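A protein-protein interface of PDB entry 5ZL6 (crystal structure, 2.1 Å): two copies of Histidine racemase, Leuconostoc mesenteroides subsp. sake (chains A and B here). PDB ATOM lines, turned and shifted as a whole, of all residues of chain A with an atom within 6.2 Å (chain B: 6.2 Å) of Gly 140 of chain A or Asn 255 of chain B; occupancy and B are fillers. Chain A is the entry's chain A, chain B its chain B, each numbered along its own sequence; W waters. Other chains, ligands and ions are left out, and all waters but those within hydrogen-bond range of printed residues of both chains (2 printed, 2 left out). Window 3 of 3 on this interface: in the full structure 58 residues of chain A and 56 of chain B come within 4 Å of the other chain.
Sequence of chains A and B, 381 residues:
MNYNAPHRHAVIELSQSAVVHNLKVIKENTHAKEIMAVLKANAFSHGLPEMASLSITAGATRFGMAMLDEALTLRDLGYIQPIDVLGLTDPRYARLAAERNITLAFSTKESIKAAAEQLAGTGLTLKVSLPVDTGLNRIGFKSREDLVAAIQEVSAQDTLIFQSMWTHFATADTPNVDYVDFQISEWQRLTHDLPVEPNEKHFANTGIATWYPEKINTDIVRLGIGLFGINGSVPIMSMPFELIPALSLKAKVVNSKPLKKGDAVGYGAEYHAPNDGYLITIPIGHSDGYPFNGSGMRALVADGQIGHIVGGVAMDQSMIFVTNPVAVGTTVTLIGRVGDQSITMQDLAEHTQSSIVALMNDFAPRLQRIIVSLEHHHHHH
OG of Ser 107 of chain A lies within hydrogen-bond range of OD1 of Asn 255 of chain B. NZ of Lys 257 of chain B lies within salt-bridge range of OD2 of Asp 133 of chain A, 3.9 Å away. The backbone carbonyl oxygen of Arg 138 of chain A is in hydrogen-bond range of the side-chain hydroxyl of Thr 281 of chain B (2.6 Å).
The backbone NH of Val 254 of chain B lies within hydrogen-bond range of the backbone carbonyl oxygen of Thr 281 of chain B. The backbone NH (N) of Thr 281 of chain B lies within hydrogen-bond range of the backbone carbonyl oxygen (O) of Asn 255 of chain B (2.9 Å). The backbone carbonyl oxygen (O) of Phe 141 of chain A sits at hydrogen-bond distance from the backbone NH (N) of Asp 133 of chain A. The backbone NH (N) of Leu 279 of chain B is in hydrogen-bond range of the backbone carbonyl oxygen (O) of Lys 257 of chain B (2.7 Å).
Val 254 of chain B touches Leu 88 of chain A (O to CD1, 3.3 Å). Leu 88 of chain A touches Asn 255 of chain B. Asn 255 of chain B touches Arg 138 of chain A. Lys 257 of chain B touches Arg 138 of chain A (NZ to O, 3.6 Å). Ile 139 of chain A touches Asn 255 of chain B (CA to OD1, 3.7 Å). N of Gly 140 of chain A touches OD1 of Asn 255 of chain B, at 3.6 Å. CG of Lys 142 of chain A touches CD of Lys 257 of chain B, 3.8 Å away.
Gly 140 of chain A touches just one residue of chain B: Asn 255 (3.6 Å). Asn 255 of chain B touches just these residues of chain A: Leu 88, Ser 107, Arg 138, Ile 139 and Gly 140. Of the printed residues of chain B, Ser 107 of chain A touches Asn 255 (2.8 Å). Printed residues of chain B within 4 Å of Leu 88 of chain A: Val 254 (3.3 Å) and Asn 255 (3.8 Å). Val 328 of chain B touches none of the printed residues of chain A. The nearest printed residue of chain B that does not touch Ser 107 of chain A is Val 254 of chain B (4.5 Å).
Of the 11 printed residues of chain B, 4 touch a printed residue of chain A. Printed residues of chain B that touch a printed residue of chain A: Val 254, Asn 255, Lys 257 and Thr 281. Of the 13 printed residues of chain A, 7 touch a printed residue of chain B. Along chain A the printed residues that touch a printed residue of chain B span positions 88 to 142. Among the printed residues, 10 pairs touch across the chains. Among the printed residues, Asp or Glu carboxylates within 4 Å of a Lys or Arg side-chain nitrogen of the other chain: Asp 133 of chain A with Lys 257 of chain B.
No position is printed for both chains.
Water W1 bridges O of Val 254 of chain B and OG of Ser 107 of chain A. Water W2 lies within hydrogen-bond range of the backbone carbonyl oxygen (O) of Gly 140 of chain A (2.6 Å) and the side-chain amide nitrogen (ND2) of Asn 255 of chain B (3.2 Å).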
ATOM      1  N   LEU A  88     -17.638  20.535   4.754  1.00  0.00           N
ATOM      2  CA  LEU A  88     -17.067  21.752   5.322  1.00  0.00           C
ATOM      3  C   LEU A  88     -16.217  21.447   6.558  1.00  0.00           C
ATOM      4  O   LEU A  88     -16.444  20.446   7.245  1.00  0.00           O
ATOM      5  CB  LEU A  88     -18.175  22.745   5.667  1.00  0.00           C
ATOM      6  CG  LEU A  88     -19.069  23.172   4.497  1.00  0.00           C
ATOM      7  CD1 LEU A  88     -20.211  24.068   4.973  1.00  0.00           C
ATOM      8  CD2 LEU A  88     -18.251  23.872   3.417  1.00  0.00           C
ATOM      9  N   PHE A 106     -14.991  25.486   1.237  1.00  0.00           N
ATOM     10  CA  PHE A 106     -15.543  26.528   2.104  1.00  0.00           C
ATOM     11  C   PHE A 106     -16.779  27.127   1.445  1.00  0.00           C
ATOM     12  O   PHE A 106     -16.846  27.217   0.222  1.00  0.00           O
ATOM     13  CB  PHE A 106     -14.506  27.621   2.385  1.00  0.00           C
ATOM     14  CG  PHE A 106     -13.378  27.173   3.270  1.00  0.00           C
ATOM     15  CD1 PHE A 106     -13.468  27.303   4.649  1.00  0.00           C
ATOM     16  CD2 PHE A 106     -12.228  26.621   2.726  1.00  0.00           C
ATOM     17  CE1 PHE A 106     -12.434  26.886   5.472  1.00  0.00           C
ATOM     18  CE2 PHE A 106     -11.190  26.203   3.542  1.00  0.00           C
ATOM     19  CZ  PHE A 106     -11.294  26.334   4.916  1.00  0.00           C
ATOM     20  N   SER A 107     -17.759  27.528   2.244  1.00  0.00           N
ATOM     21  CA  SER A 107     -19.013  28.034   1.688  1.00  0.00           C
ATOM     22  C   SER A 107     -19.301  29.473   2.113  1.00  0.00           C
ATOM     23  O   SER A 107     -20.391  29.997   1.873  1.00  0.00           O
ATOM     24  CB  SER A 107     -20.182  27.136   2.098  1.00  0.00           C
ATOM     25  OG  SER A 107     -20.425  27.210   3.494  1.00  0.00           O
ATOM     26  N   THR A 108     -18.315  30.116   2.725  1.00  0.00           N
ATOM     27  CA  THR A 108     -18.547  31.410   3.348  1.00  0.00           C
ATOM     28  C   THR A 108     -17.281  32.274   3.295  1.00  0.00           C
ATOM     29  O   THR A 108     -16.187  31.799   3.590  1.00  0.00           O
ATOM     30  CB  THR A 108     -19.043  31.205   4.805  1.00  0.00           C
ATOM     31  OG1 THR A 108     -20.467  31.377   4.863  1.00  0.00           O
ATOM     32  CG2 THR A 108     -18.397  32.162   5.757  1.00  0.00           C
ATOM     33  N   LEU A 130     -14.625  26.081  -3.733  1.00  0.00           N
ATOM     34  CA  LEU A 130     -15.848  26.815  -3.429  1.00  0.00           C
ATOM     35  C   LEU A 130     -17.036  26.130  -4.089  1.00  0.00           C
ATOM     36  O   LEU A 130     -17.292  26.331  -5.277  1.00  0.00           O
ATOM     37  CB  LEU A 130     -15.755  28.274  -3.901  1.00  0.00           C
ATOM     38  CG  LEU A 130     -14.564  29.166  -3.509  1.00  0.00           C
ATOM     39  CD1 LEU A 130     -14.824  30.607  -3.928  1.00  0.00           C
ATOM     40  CD2 LEU A 130     -14.251  29.107  -2.023  1.00  0.00           C
ATOM     41  N   PRO A 131     -17.753  25.294  -3.329  1.00  0.00           N
ATOM     42  CA  PRO A 131     -18.980  24.740  -3.898  1.00  0.00           C
ATOM     43  C   PRO A 131     -19.996  25.846  -4.186  1.00  0.00           C
ATOM     44  O   PRO A 131     -20.120  26.799  -3.414  1.00  0.00           O
ATOM     45  CB  PRO A 131     -19.485  23.793  -2.808  1.00  0.00           C
ATOM     46  CG  PRO A 131     -18.807  24.238  -1.555  1.00  0.00           C
ATOM     47  CD  PRO A 131     -17.482  24.786  -1.974  1.00  0.00           C
ATOM     48  N   VAL A 132     -20.693  25.720  -5.309  1.00  0.00           N
ATOM     49  CA  VAL A 132     -21.809  26.598  -5.629  1.00  0.00           C
ATOM     50  C   VAL A 132     -23.084  25.793  -5.477  1.00  0.00           C
ATOM     51  O   VAL A 132     -23.217  24.729  -6.073  1.00  0.00           O
ATOM     52  CB  VAL A 132     -21.720  27.160  -7.062  1.00  0.00           C
ATOM     53  CG1 VAL A 132     -22.970  27.956  -7.402  1.00  0.00           C
ATOM     54  CG2 VAL A 132     -20.468  28.008  -7.232  1.00  0.00           C
ATOM     55  N   ASP A 133     -24.014  26.283  -4.668  1.00  0.00           N
ATOM     56  CA  ASP A 133     -25.300  25.613  -4.525  1.00  0.00           C
ATOM     57  C   ASP A 133     -26.221  25.958  -5.695  1.00  0.00           C
ATOM     58  O   ASP A 133     -26.592  27.113  -5.883  1.00  0.00           O
ATOM     59  CB  ASP A 133     -25.958  25.995  -3.203  1.00  0.00           C
ATOM     60  CG  ASP A 133     -27.129  25.102  -2.862  1.00  0.00           C
ATOM     61  OD1 ASP A 133     -27.729  24.520  -3.792  1.00  0.00           O
ATOM     62  OD2 ASP A 133     -27.445  24.980  -1.661  1.00  0.00           O
ATOM     63  N   ARG A 138     -27.759  21.885   0.036  1.00  0.00           N
ATOM     64  CA  ARG A 138     -27.109  21.399   1.249  1.00  0.00           C
ATOM     65  C   ARG A 138     -25.980  22.346   1.669  1.00  0.00           C
ATOM     66  O   ARG A 138     -25.948  22.796   2.813  1.00  0.00           O
ATOM     67  CB  ARG A 138     -26.587  19.966   1.074  1.00  0.00           C
ATOM     68  CG  ARG A 138     -25.588  19.762  -0.041  1.00  0.00           C
ATOM     69  CD  ARG A 138     -24.339  19.044   0.465  1.00  0.00           C
ATOM     70  NE  ARG A 138     -24.525  17.603   0.627  1.00  0.00           N
ATOM     71  CZ  ARG A 138     -24.032  16.682  -0.199  1.00  0.00           C
ATOM     72  NH1 ARG A 138     -23.325  17.047  -1.262  1.00  0.00           N
ATOM     73  NH2 ARG A 138     -24.246  15.391   0.033  1.00  0.00           N
ATOM     74  N   ILE A 139     -25.059  22.651   0.755  1.00  0.00           N
ATOM     75  CA  ILE A 139     -23.982  23.611   1.020  1.00  0.00           C
ATOM     76  C   ILE A 139     -23.569  24.352  -0.241  1.00  0.00           C
ATOM     77  O   ILE A 139     -23.827  23.899  -1.359  1.00  0.00           O
ATOM     78  CB  ILE A 139     -22.694  22.950   1.596  1.00  0.00           C
ATOM     79  CG1 ILE A 139     -21.988  22.119   0.523  1.00  0.00           C
ATOM     80  CG2 ILE A 139     -22.974  22.150   2.864  1.00  0.00           C
ATOM     81  CD1 ILE A 139     -20.601  21.657   0.933  1.00  0.00           C
ATOM     82  N   GLY A 140     -22.898  25.484  -0.056  1.00  0.00           N
ATOM     83  CA  GLY A 140     -22.340  26.220  -1.172  1.00  0.00           C
ATOM     84  C   GLY A 140     -22.857  27.639  -1.258  1.00  0.00           C
ATOM     85  O   GLY A 140     -23.789  28.024  -0.548  1.00  0.00           O
ATOM     86  N   PHE A 141     -22.245  28.423  -2.135  1.00  0.00           N
ATOM     87  CA  PHE A 141     -22.654  29.806  -2.311  1.00  0.00           C
ATOM     88  C   PHE A 141     -23.999  29.899  -3.038  1.00  0.00           C
ATOM     89  O   PHE A 141     -24.281  29.130  -3.955  1.00  0.00           O
ATOM     90  CB  PHE A 141     -21.555  30.574  -3.042  1.00  0.00           C
ATOM     91  CG  PHE A 141     -20.333  30.783  -2.200  1.00  0.00           C
ATOM     92  CD1 PHE A 141     -19.344  29.812  -2.136  1.00  0.00           C
ATOM     93  CD2 PHE A 141     -20.195  31.932  -1.429  1.00  0.00           C
ATOM     94  CE1 PHE A 141     -18.229  29.992  -1.340  1.00  0.00           C
ATOM     95  CE2 PHE A 141     -19.086  32.117  -0.630  1.00  0.00           C
ATOM     96  CZ  PHE A 141     -18.099  31.147  -0.586  1.00  0.00           C
ATOM     97  N   LYS A 142     -24.831  30.839  -2.599  1.00  0.00           N
ATOM     98  CA  LYS A 142     -26.207  30.931  -3.072  1.00  0.00           C
ATOM     99  C   LYS A 142     -26.464  32.159  -3.940  1.00  0.00           C
ATOM    100  O   LYS A 142     -27.573  32.351  -4.433  1.00  0.00           O
ATOM    101  CB  LYS A 142     -27.163  30.925  -1.877  1.00  0.00           C
ATOM    102  CG  LYS A 142     -27.319  29.553  -1.223  1.00  0.00           C
ATOM    103  CD  LYS A 142     -28.101  28.603  -2.121  1.00  0.00           C
ATOM    104  CE  LYS A 142     -29.541  29.073  -2.300  1.00  0.00           C
ATOM    105  NZ  LYS A 142     -30.384  28.069  -3.013  1.00  0.00           N
ATOM    106  N   LYS B 252     -22.816  20.341  15.259  1.00  0.00           N
ATOM    107  CA  LYS B 252     -22.877  21.778  15.040  1.00  0.00           C
ATOM    108  C   LYS B 252     -23.123  22.135  13.582  1.00  0.00           C
ATOM    109  O   LYS B 252     -22.572  21.517  12.668  1.00  0.00           O
ATOM    110  CB  LYS B 252     -21.594  22.445  15.532  1.00  0.00           C
ATOM    111  CG  LYS B 252     -21.523  22.545  17.037  1.00  0.00           C
ATOM    112  CD  LYS B 252     -20.212  23.150  17.497  1.00  0.00           C
ATOM    113  CE  LYS B 252     -20.252  23.430  18.980  1.00  0.00           C
ATOM    114  NZ  LYS B 252     -21.281  24.451  19.284  1.00  0.00           N
ATOM    115  N   VAL B 253     -23.973  23.139  13.387  1.00  0.00           N
ATOM    116  CA  VAL B 253     -24.284  23.675  12.073  1.00  0.00           C
ATOM    117  C   VAL B 253     -23.024  24.067  11.310  1.00  0.00           C
ATOM    118  O   VAL B 253     -22.187  24.804  11.831  1.00  0.00           O
ATOM    119  CB  VAL B 253     -25.191  24.910  12.191  1.00  0.00           C
ATOM    120  CG1 VAL B 253     -25.369  25.558  10.838  1.00  0.00           C
ATOM    121  CG2 VAL B 253     -26.530  24.533  12.812  1.00  0.00           C
ATOM    122  N   VAL B 254     -22.893  23.587  10.075  1.00  0.00           N
ATOM    123  CA  VAL B 254     -21.733  23.926   9.249  1.00  0.00           C
ATOM    124  C   VAL B 254     -22.094  24.894   8.120  1.00  0.00           C
ATOM    125  O   VAL B 254     -21.251  25.660   7.650  1.00  0.00           O
ATOM    126  CB  VAL B 254     -21.081  22.668   8.637  1.00  0.00           C
ATOM    127  CG1 VAL B 254     -20.444  21.808   9.730  1.00  0.00           C
ATOM    128  CG2 VAL B 254     -22.096  21.869   7.825  1.00  0.00           C
ATOM    129  N   ASN B 255     -23.350  24.859   7.691  1.00  0.00           N
ATOM    130  CA  ASN B 255     -23.830  25.738   6.632  1.00  0.00           C
ATOM    131  C   ASN B 255     -25.200  26.287   7.004  1.00  0.00           C
ATOM    132  O   ASN B 255     -26.051  25.541   7.485  1.00  0.00           O
ATOM    133  CB  ASN B 255     -23.888  24.986   5.302  1.00  0.00           C
ATOM    134  CG  ASN B 255     -24.015  25.909   4.112  1.00  0.00           C
ATOM    135  OD1 ASN B 255     -23.023  26.239   3.462  1.00  0.00           O
ATOM    136  ND2 ASN B 255     -25.239  26.326   3.810  1.00  0.00           N
ATOM    137  N   SER B 256     -25.413  27.584   6.800  1.00  0.00           N
ATOM    138  CA  SER B 256     -26.675  28.210   7.188  1.00  0.00           C
ATOM    139  C   SER B 256     -27.093  29.322   6.230  1.00  0.00           C
ATOM    140  O   SER B 256     -26.334  30.255   5.968  1.00  0.00           O
ATOM    141  CB  SER B 256     -26.580  28.764   8.608  1.00  0.00           C
ATOM    142  OG  SER B 256     -27.836  29.270   9.029  1.00  0.00           O
ATOM    143  N   LYS B 257     -28.319  29.219   5.730  1.00  0.00           N
ATOM    144  CA  LYS B 257     -28.816  30.108   4.687  1.00  0.00           C
ATOM    145  C   LYS B 257     -30.321  30.308   4.804  1.00  0.00           C
ATOM    146  O   LYS B 257     -31.013  29.485   5.394  1.00  0.00           O
ATOM    147  CB  LYS B 257     -28.483  29.534   3.304  1.00  0.00           C
ATOM    148  CG  LYS B 257     -29.035  28.122   3.082  1.00  0.00           C
ATOM    149  CD  LYS B 257     -28.864  27.661   1.643  1.00  0.00           C
ATOM    150  CE  LYS B 257     -29.391  26.239   1.434  1.00  0.00           C
ATOM    151  NZ  LYS B 257     -28.535  25.192   2.080  1.00  0.00           N
ATOM    152  N   LEU B 279     -32.410  27.325   6.298  1.00  0.00           N
ATOM    153  CA  LEU B 279     -31.999  25.933   6.189  1.00  0.00           C
ATOM    154  C   LEU B 279     -30.645  25.702   6.845  1.00  0.00           C
ATOM    155  O   LEU B 279     -29.636  26.325   6.507  1.00  0.00           O
ATOM    156  CB  LEU B 279     -31.962  25.485   4.730  1.00  0.00           C
ATOM    157  CG  LEU B 279     -31.958  23.963   4.572  1.00  0.00           C
ATOM    158  CD1 LEU B 279     -33.342  23.379   4.879  1.00  0.00           C
ATOM    159  CD2 LEU B 279     -31.486  23.557   3.190  1.00  0.00           C
ATOM    160  N   ILE B 280     -30.653  24.769   7.781  1.00  0.00           N
ATOM    161  CA  ILE B 280     -29.543  24.503   8.671  1.00  0.00           C
ATOM    162  C   ILE B 280     -28.918  23.152   8.327  1.00  0.00           C
ATOM    163  O   ILE B 280     -29.566  22.124   8.486  1.00  0.00           O
ATOM    164  CB  ILE B 280     -30.053  24.532  10.141  1.00  0.00           C
ATOM    165  CG1 ILE B 280     -29.893  25.929  10.742  1.00  0.00           C
ATOM    166  CG2 ILE B 280     -29.402  23.472  10.987  1.00  0.00           C
ATOM    167  CD1 ILE B 280     -28.610  26.574  10.405  1.00  0.00           C
ATOM    168  N   THR B 281     -27.677  23.146   7.836  1.00  0.00           N
ATOM    169  CA  THR B 281     -27.026  21.885   7.453  1.00  0.00           C
ATOM    170  C   THR B 281     -26.033  21.386   8.512  1.00  0.00           C
ATOM    171  O   THR B 281     -25.141  22.124   8.931  1.00  0.00           O
ATOM    172  CB  THR B 281     -26.279  22.014   6.104  1.00  0.00           C
ATOM    173  OG1 THR B 281     -27.175  22.498   5.093  1.00  0.00           O
ATOM    174  CG2 THR B 281     -25.720  20.658   5.668  1.00  0.00           C
ATOM    175  N   ILE B 282     -26.193  20.131   8.938  1.00  0.00           N
ATOM    176  CA  ILE B 282     -25.323  19.549   9.962  1.00  0.00           C
ATOM    177  C   ILE B 282     -24.528  18.361   9.423  1.00  0.00           C
ATOM    178  O   ILE B 282     -24.986  17.668   8.506  1.00  0.00           O
ATOM    179  CB  ILE B 282     -26.117  19.095  11.211  1.00  0.00           C
ATOM    180  CG1 ILE B 282     -27.248  18.141  10.830  1.00  0.00           C
ATOM    181  CG2 ILE B 282     -26.665  20.295  11.967  1.00  0.00           C
ATOM    182  CD1 ILE B 282     -27.953  17.540  12.028  1.00  0.00           C
ATOM    183  N   VAL B 328     -23.991  29.570  12.168  1.00  0.00           N
ATOM    184  CA  VAL B 328     -23.002  28.515  12.024  1.00  0.00           C
ATOM    185  C   VAL B 328     -22.330  28.239  13.370  1.00  0.00           C
ATOM    186  O   VAL B 328     -21.976  29.171  14.093  1.00  0.00           O
ATOM    187  CB  VAL B 328     -21.944  28.909  10.974  1.00  0.00           C
ATOM    188  CG1 VAL B 328     -20.726  27.996  11.044  1.00  0.00           C
ATOM    189  CG2 VAL B 328     -22.557  28.918   9.579  1.00  0.00           C
HETATM  190  O   HOH W   1     -20.596  27.787   6.396  1.00  0.00           O
HETATM  191  O   HOH W   2     -25.132  28.696   1.625  1.00  0.00           O
